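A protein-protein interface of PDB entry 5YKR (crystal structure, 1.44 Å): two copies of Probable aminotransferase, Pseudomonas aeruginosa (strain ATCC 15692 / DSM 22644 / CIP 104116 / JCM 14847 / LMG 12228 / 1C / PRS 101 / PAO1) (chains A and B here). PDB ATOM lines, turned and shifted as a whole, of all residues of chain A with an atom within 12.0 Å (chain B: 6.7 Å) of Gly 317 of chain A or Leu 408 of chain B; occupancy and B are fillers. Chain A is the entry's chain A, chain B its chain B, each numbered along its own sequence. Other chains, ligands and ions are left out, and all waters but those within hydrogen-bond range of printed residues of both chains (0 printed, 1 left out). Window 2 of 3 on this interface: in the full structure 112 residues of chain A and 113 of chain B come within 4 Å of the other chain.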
ATOM      1  N   PRO A 312      -0.641   8.408 -16.259  1.00  0.00           N
ATOM      2  CA  PRO A 312       0.088   9.616 -16.616  1.00  0.00           C
ATOM      3  C   PRO A 312       1.595   9.524 -16.352  1.00  0.00           C
ATOM      4  O   PRO A 312       2.073   8.742 -15.529  1.00  0.00           O
ATOM      5  CB  PRO A 312      -0.487  10.657 -15.686  1.00  0.00           C
ATOM      6  CG  PRO A 312      -1.848  10.188 -15.347  1.00  0.00           C
ATOM      7  CD  PRO A 312      -1.719   8.680 -15.273  1.00  0.00           C
ATOM      8  N   HIS A 313       2.326  10.321 -17.126  1.00  0.00           N
ATOM      9  CA  HIS A 313       3.761  10.466 -16.854  1.00  0.00           C
ATOM     10  C   HIS A 313       3.959  10.864 -15.389  1.00  0.00           C
ATOM     11  O   HIS A 313       3.193  11.636 -14.802  1.00  0.00           O
ATOM     12  CB  HIS A 313       4.346  11.533 -17.796  1.00  0.00           C
ATOM     13  CG  HIS A 313       4.339  11.076 -19.205  1.00  0.00           C
ATOM     14  ND1 HIS A 313       5.204  10.105 -19.670  1.00  0.00           N
ATOM     15  CD2 HIS A 313       3.502  11.397 -20.235  1.00  0.00           C
ATOM     16  CE1 HIS A 313       4.931   9.874 -20.941  1.00  0.00           C
ATOM     17  NE2 HIS A 313       3.884  10.619 -21.301  1.00  0.00           N
ATOM     18  N   PHE A 314       4.990  10.290 -14.796  1.00  0.00           N
ATOM     19  CA  PHE A 314       5.178  10.422 -13.328  1.00  0.00           C
ATOM     20  C   PHE A 314       5.505  11.852 -12.970  1.00  0.00           C
ATOM     21  O   PHE A 314       6.288  12.515 -13.664  1.00  0.00           O
ATOM     22  CB  PHE A 314       6.314   9.484 -12.893  1.00  0.00           C
ATOM     23  CG  PHE A 314       6.324   9.132 -11.449  1.00  0.00           C
ATOM     24  CD1 PHE A 314       5.413   8.192 -10.937  1.00  0.00           C
ATOM     25  CD2 PHE A 314       7.225   9.711 -10.611  1.00  0.00           C
ATOM     26  CE1 PHE A 314       5.445   7.833  -9.615  1.00  0.00           C
ATOM     27  CE2 PHE A 314       7.274   9.376  -9.261  1.00  0.00           C
ATOM     28  CZ  PHE A 314       6.393   8.438  -8.766  1.00  0.00           C
ATOM     29  N   ARG A 315       4.941  12.331 -11.875  1.00  0.00           N
ATOM     30  CA  ARG A 315       5.095  13.702 -11.456  1.00  0.00           C
ATOM     31  C   ARG A 315       6.081  13.771 -10.280  1.00  0.00           C
ATOM     32  O   ARG A 315       6.179  12.831  -9.460  1.00  0.00           O
ATOM     33  CB  ARG A 315       3.720  14.279 -11.071  1.00  0.00           C
ATOM     34  CG  ARG A 315       2.748  14.374 -12.258  1.00  0.00           C
ATOM     35  CD  ARG A 315       1.322  14.848 -11.828  1.00  0.00           C
ATOM     36  NE  ARG A 315       0.515  15.427 -12.929  1.00  0.00           N
ATOM     37  CZ  ARG A 315      -0.346  14.763 -13.720  1.00  0.00           C
ATOM     38  NH1 ARG A 315      -0.579  13.443 -13.550  1.00  0.00           N
ATOM     39  NH2 ARG A 315      -1.059  15.449 -14.673  1.00  0.00           N
ATOM     40  N   PRO A 316       6.811  14.883 -10.170  1.00  0.00           N
ATOM     41  CA  PRO A 316       7.770  15.044  -9.085  1.00  0.00           C
ATOM     42  C   PRO A 316       7.140  14.879  -7.736  1.00  0.00           C
ATOM     43  O   PRO A 316       6.103  15.512  -7.447  1.00  0.00           O
ATOM     44  CB  PRO A 316       8.227  16.494  -9.242  1.00  0.00           C
ATOM     45  CG  PRO A 316       7.781  16.964 -10.585  1.00  0.00           C
ATOM     46  CD  PRO A 316       6.735  16.062 -11.066  1.00  0.00           C
ATOM     47  N   GLY A 317       7.692  14.001  -6.915  1.00  0.00           N
ATOM     48  CA  GLY A 317       7.162  13.772  -5.580  1.00  0.00           C
ATOM     49  C   GLY A 317       5.933  12.879  -5.493  1.00  0.00           C
ATOM     50  O   GLY A 317       5.433  12.642  -4.414  1.00  0.00           O
ATOM     51  N   GLN A 318       5.463  12.354  -6.617  1.00  0.00           N
ATOM     52  CA  GLN A 318       4.346  11.408  -6.627  1.00  0.00           C
ATOM     53  C   GLN A 318       4.707  10.139  -5.884  1.00  0.00           C
ATOM     54  O   GLN A 318       5.876   9.751  -5.847  1.00  0.00           O
ATOM     55  CB  GLN A 318       3.997  11.079  -8.096  1.00  0.00           C
ATOM     56  CG  GLN A 318       2.865  10.081  -8.304  1.00  0.00           C
ATOM     57  CD  GLN A 318       2.491   9.884  -9.749  1.00  0.00           C
ATOM     58  OE1 GLN A 318       2.789  10.751 -10.602  1.00  0.00           O
ATOM     59  NE2 GLN A 318       1.826   8.756 -10.045  1.00  0.00           N
ATOM     60  N   ALA A 319       3.727   9.467  -5.281  1.00  0.00           N
ATOM     61  CA  ALA A 319       3.963   8.195  -4.652  1.00  0.00           C
ATOM     62  C   ALA A 319       4.435   7.181  -5.686  1.00  0.00           C
ATOM     63  O   ALA A 319       3.806   6.988  -6.729  1.00  0.00           O
ATOM     64  CB  ALA A 319       2.717   7.691  -3.948  1.00  0.00           C
ATOM     65  N   ILE A 320       5.523   6.491  -5.360  1.00  0.00           N
ATOM     66  CA  ILE A 320       6.056   5.417  -6.207  1.00  0.00           C
ATOM     67  C   ILE A 320       5.020   4.310  -6.430  1.00  0.00           C
ATOM     68  O   ILE A 320       4.270   3.976  -5.560  1.00  0.00           O
ATOM     69  CB  ILE A 320       7.386   4.844  -5.541  1.00  0.00           C
ATOM     70  CG1 ILE A 320       8.542   5.480  -6.300  1.00  0.00           C
ATOM     71  CG2 ILE A 320       7.496   3.330  -5.387  1.00  0.00           C
ATOM     72  CD1 ILE A 320       8.703   6.885  -6.068  1.00  0.00           C
ATOM     73  N   ASN A 321       5.021   3.727  -7.630  1.00  0.00           N
ATOM     74  CA  ASN A 321       4.160   2.581  -7.931  1.00  0.00           C
ATOM     75  C   ASN A 321       4.659   1.906  -9.205  1.00  0.00           C
ATOM     76  O   ASN A 321       4.998   2.564 -10.163  1.00  0.00           O
ATOM     77  CB  ASN A 321       2.701   3.017  -8.146  1.00  0.00           C
ATOM     78  CG  ASN A 321       1.689   1.927  -7.884  1.00  0.00           C
ATOM     79  OD1 ASN A 321       2.005   0.745  -7.963  1.00  0.00           O
ATOM     80  ND2 ASN A 321       0.447   2.340  -7.581  1.00  0.00           N
ATOM     81  N   PHE A 323       2.504  -0.062 -10.776  1.00  0.00           N
ATOM     82  CA  PHE A 323       1.261  -0.104 -11.582  1.00  0.00           C
ATOM     83  C   PHE A 323       0.960  -1.508 -12.169  1.00  0.00           C
ATOM     84  O   PHE A 323       0.182  -1.647 -13.090  1.00  0.00           O
ATOM     85  CB  PHE A 323       1.240   0.971 -12.687  1.00  0.00           C
ATOM     86  CG  PHE A 323       1.543   2.353 -12.168  1.00  0.00           C
ATOM     87  CD1 PHE A 323       0.610   3.054 -11.407  1.00  0.00           C
ATOM     88  CD2 PHE A 323       2.729   2.982 -12.510  1.00  0.00           C
ATOM     89  CE1 PHE A 323       0.855   4.337 -10.964  1.00  0.00           C
ATOM     90  CE2 PHE A 323       2.973   4.253 -12.058  1.00  0.00           C
ATOM     91  CZ  PHE A 323       2.054   4.936 -11.261  1.00  0.00           C
ATOM     92  N   LEU B   9       5.737  20.330   5.698  1.00  0.00           N
ATOM     93  CA  LEU B   9       5.704  20.002   4.272  1.00  0.00           C
ATOM     94  C   LEU B   9       5.956  21.201   3.352  1.00  0.00           C
ATOM     95  O   LEU B   9       6.464  21.039   2.271  1.00  0.00           O
ATOM     96  CB  LEU B   9       4.416  19.261   3.901  1.00  0.00           C
ATOM     97  CG  LEU B   9       4.295  17.856   4.545  1.00  0.00           C
ATOM     98  CD1 LEU B   9       2.968  17.199   4.190  1.00  0.00           C
ATOM     99  CD2 LEU B   9       5.452  16.928   4.175  1.00  0.00           C
ATOM    100  N   ALA B  10       5.647  22.406   3.785  1.00  0.00           N
ATOM    101  CA  ALA B  10       6.008  23.586   3.004  1.00  0.00           C
ATOM    102  C   ALA B  10       7.518  23.788   2.936  1.00  0.00           C
ATOM    103  O   ALA B  10       8.038  24.212   1.897  1.00  0.00           O
ATOM    104  CB  ALA B  10       5.347  24.825   3.579  1.00  0.00           C
ATOM    105  N   VAL B  12       9.637  21.310   3.170  1.00  0.00           N
ATOM    106  CA  VAL B  12      10.059  20.220   2.274  1.00  0.00           C
ATOM    107  C   VAL B  12       9.864  20.622   0.803  1.00  0.00           C
ATOM    108  O   VAL B  12      10.744  20.441  -0.036  1.00  0.00           O
ATOM    109  CB  VAL B  12       9.318  18.892   2.577  1.00  0.00           C
ATOM    110  CG1 VAL B  12       9.719  17.804   1.619  1.00  0.00           C
ATOM    111  CG2 VAL B  12       9.589  18.445   4.004  1.00  0.00           C
ATOM    112  N   GLU B  13       8.695  21.148   0.496  1.00  0.00           N
ATOM    113  CA  GLU B  13       8.415  21.640  -0.860  1.00  0.00           C
ATOM    114  C   GLU B  13       9.432  22.708  -1.324  1.00  0.00           C
ATOM    115  O   GLU B  13       9.897  22.681  -2.451  1.00  0.00           O
ATOM    116  CB  GLU B  13       6.985  22.173  -0.894  1.00  0.00           C
ATOM    117  CG  GLU B  13       6.613  22.976  -2.090  1.00  0.00           C
ATOM    118  CD  GLU B  13       6.321  22.146  -3.294  1.00  0.00           C
ATOM    119  OE1 GLU B  13       6.638  20.923  -3.280  1.00  0.00           O
ATOM    120  OE2 GLU B  13       5.708  22.725  -4.228  1.00  0.00           O
ATOM    121  N   PHE B  16      12.727  21.063  -1.972  1.00  0.00           N
ATOM    122  CA  PHE B  16      12.594  20.192  -3.148  1.00  0.00           C
ATOM    123  C   PHE B  16      12.645  20.997  -4.416  1.00  0.00           C
ATOM    124  O   PHE B  16      13.311  20.627  -5.352  1.00  0.00           O
ATOM    125  CB  PHE B  16      11.278  19.375  -3.051  1.00  0.00           C
ATOM    126  CG  PHE B  16      11.088  18.341  -4.142  1.00  0.00           C
ATOM    127  CD1 PHE B  16      12.067  17.483  -4.469  1.00  0.00           C
ATOM    128  CD2 PHE B  16       9.831  18.195  -4.764  1.00  0.00           C
ATOM    129  CE1 PHE B  16      11.880  16.528  -5.456  1.00  0.00           C
ATOM    130  CE2 PHE B  16       9.648  17.222  -5.765  1.00  0.00           C
ATOM    131  CZ  PHE B  16      10.661  16.398  -6.075  1.00  0.00           C
ATOM    132  N   PRO B  54      13.920  10.850  -8.723  1.00  0.00           N
ATOM    133  CA  PRO B  54      13.519  12.224  -8.463  1.00  0.00           C
ATOM    134  C   PRO B  54      14.369  13.125  -9.370  1.00  0.00           C
ATOM    135  O   PRO B  54      15.401  12.721  -9.907  1.00  0.00           O
ATOM    136  CB  PRO B  54      13.833  12.373  -7.000  1.00  0.00           C
ATOM    137  CG  PRO B  54      15.055  11.558  -6.820  1.00  0.00           C
ATOM    138  CD  PRO B  54      14.775  10.343  -7.677  1.00  0.00           C
ATOM    139  N   ASN B 406       5.740   8.688   2.326  1.00  0.00           N
ATOM    140  CA  ASN B 406       5.327   9.976   1.797  1.00  0.00           C
ATOM    141  C   ASN B 406       6.150  10.325   0.601  1.00  0.00           C
ATOM    142  O   ASN B 406       7.402  10.420   0.715  1.00  0.00           O
ATOM    143  CB  ASN B 406       5.447  11.060   2.879  1.00  0.00           C
ATOM    144  CG  ASN B 406       5.004  12.421   2.374  1.00  0.00           C
ATOM    145  OD1 ASN B 406       5.797  13.193   1.797  1.00  0.00           O
ATOM    146  ND2 ASN B 406       3.726  12.695   2.510  1.00  0.00           N
ATOM    147  N   GLY B 407       5.490  10.511  -0.532  1.00  0.00           N
ATOM    148  CA  GLY B 407       6.188  10.711  -1.801  1.00  0.00           C
ATOM    149  C   GLY B 407       7.076  11.945  -1.842  1.00  0.00           C
ATOM    150  O   GLY B 407       8.192  11.926  -2.398  1.00  0.00           O
ATOM    151  N   LEU B 408       6.589  13.028  -1.260  1.00  0.00           N
ATOM    152  CA  LEU B 408       7.282  14.307  -1.315  1.00  0.00           C
ATOM    153  C   LEU B 408       8.560  14.299  -0.457  1.00  0.00           C
ATOM    154  O   LEU B 408       9.622  14.712  -0.930  1.00  0.00           O
ATOM    155  CB  LEU B 408       6.340  15.427  -0.881  1.00  0.00           C
ATOM    156  CG  LEU B 408       6.996  16.791  -0.646  1.00  0.00           C
ATOM    157  CD1 LEU B 408       7.653  17.345  -1.890  1.00  0.00           C
ATOM    158  CD2 LEU B 408       5.997  17.786  -0.065  1.00  0.00           C
ATOM    159  N   ILE B 409       8.466  13.803   0.782  1.00  0.00           N
ATOM    160  CA  ILE B 409       9.632  13.737   1.660  1.00  0.00           C
ATOM    161  C   ILE B 409      10.642  12.799   1.030  1.00  0.00           C
ATOM    162  O   ILE B 409      11.842  13.106   0.962  1.00  0.00           O
ATOM    163  CB  ILE B 409       9.275  13.284   3.094  1.00  0.00           C
ATOM    164  CG1 ILE B 409       8.380  14.309   3.784  1.00  0.00           C
ATOM    165  CG2 ILE B 409      10.544  13.020   3.890  1.00  0.00           C
ATOM    166  CD1 ILE B 409       7.702  13.752   5.023  1.00  0.00           C
ATOM    167  N   GLU B 410      10.167  11.642   0.558  1.00  0.00           N
ATOM    168  CA  GLU B 410      11.063  10.678  -0.082  1.00  0.00           C
ATOM    169  C   GLU B 410      11.807  11.274  -1.294  1.00  0.00           C
ATOM    170  O   GLU B 410      13.027  11.143  -1.393  1.00  0.00           O
ATOM    171  CB  GLU B 410      10.288   9.416  -0.488  1.00  0.00           C
ATOM    172  CG  GLU B 410       9.835   8.643   0.726  1.00  0.00           C
ATOM    173  CD  GLU B 410       8.830   7.537   0.445  1.00  0.00           C
ATOM    174  OE1 GLU B 410       8.762   6.991  -0.685  1.00  0.00           O
ATOM    175  OE2 GLU B 410       8.086   7.189   1.374  1.00  0.00           O
ATOM    176  N   ALA B 411      11.088  11.982  -2.164  1.00  0.00           N
ATOM    177  CA  ALA B 411      11.701  12.573  -3.328  1.00  0.00           C
ATOM    178  C   ALA B 411      12.734  13.623  -2.932  1.00  0.00           C
ATOM    179  O   ALA B 411      13.824  13.688  -3.512  1.00  0.00           O
ATOM    180  CB  ALA B 411      10.635  13.159  -4.239  1.00  0.00           C
ATOM    181  N   CYS B 412      12.401  14.441  -1.952  1.00  0.00           N
ATOM    182  CA  CYS B 412      13.326  15.447  -1.496  1.00  0.00           C
ATOM    183  C   CYS B 412      14.623  14.899  -0.929  1.00  0.00           C
ATOM    184  O   CYS B 412      15.700  15.345  -1.306  1.00  0.00           O
ATOM    185  CB  CYS B 412      12.647  16.324  -0.459  1.00  0.00           C
ATOM    186  SG  CYS B 412      13.579  17.824  -0.052  1.00  0.00           S
ATOM    187  N   LEU B 413      14.527  13.911  -0.046  1.00  0.00           N
ATOM    188  CA  LEU B 413      15.737  13.307   0.531  1.00  0.00           C
ATOM    189  C   LEU B 413      16.554  12.630  -0.564  1.00  0.00           C
ATOM    190  O   LEU B 413      17.779  12.762  -0.594  1.00  0.00           O
ATOM    191  CB  LEU B 413      15.372  12.268   1.628  1.00  0.00           C
ATOM    192  CG  LEU B 413      14.698  12.741   2.910  1.00  0.00           C
ATOM    193  CD1 LEU B 413      14.474  11.579   3.836  1.00  0.00           C
ATOM    194  CD2 LEU B 413      15.470  13.817   3.525  1.00  0.00           C
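O of Gly 407 of chain B sits close to O of Gly 317 of chain A (3.5 Å).
The backbone carbonyl oxygen of Gly 317 of chain A sits at hydrogen-bond distance from the backbone NH of Leu 408 of chain B, at 3.4 Å.
N of Leu 408 of chain B is in hydrogen-bond range of OD1 of Asn 406 of chain B (3.2 Å).
Among the printed residues, pairs that only touch across the chains: Pro 316 of chain A with Phe 16 of chain B (3.8 Å), Gly 317 of chain A with Phe 16 of chain B (3.9 Å) and Gly 317 of chain A with Ala 411 of chain B (3.8 Å).
Gly 317 of chain A touches just these residues of chain B: Phe 16, Gly 407, Leu 408 and Ala 411.
Leu 408 of chain B touches just one residue of chain A: Gly 317.
No residue of chain A comes within 4 Å of Val 12 of chain B.
No residue of chain A comes within 4 Å of Glu 13 of chain B.
Printed residues of chain A within 4 Å of Phe 16 of chain B: Pro 316 and Gly 317.
No residue of chain A comes within 4 Å of Asn 406 of chain B.
Gly 407 of chain B touches just one residue of chain A: Gly 317 (3.1 Å).
Of the printed residues of chain A, Ala 411 of chain B touches Gly 317 (3.8 Å).
No residue of chain A comes within 4 Å of Cys 412 of chain B.
Of the printed residues of chain B, Pro 316 of chain A touches Phe 16 (3.8 Å).
Ala 10 of chain B touches none of the printed residues of chain A.
The nearest residue of chain A that does not touch Leu 408 of chain B is Gln 318 of chain A (5.5 Å).
The nearest printed residue of chain B that does not touch Pro 316 of chain A is Ala 411 of chain B (5.2 Å).
Hydrophobic or aromatic side chains of chain A within 4 Å of the printed part of chain B: Pro 316.
Printed residues of chain B that touch a printed residue of chain A: Phe 16, Gly 407, Leu 408 and Ala 411.
Along chain B the printed residues that touch a printed residue of chain A span positions 16 to 411.
Among the printed residues, no Asp or Glu carboxylate lies within 4 Å of a Lys or Arg side-chain nitrogen of the other chain.
No position is printed for both chains.
Of the 5 pairs that touch across the chains among the printed residues, none has its exchanged pair printed and touching as well.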
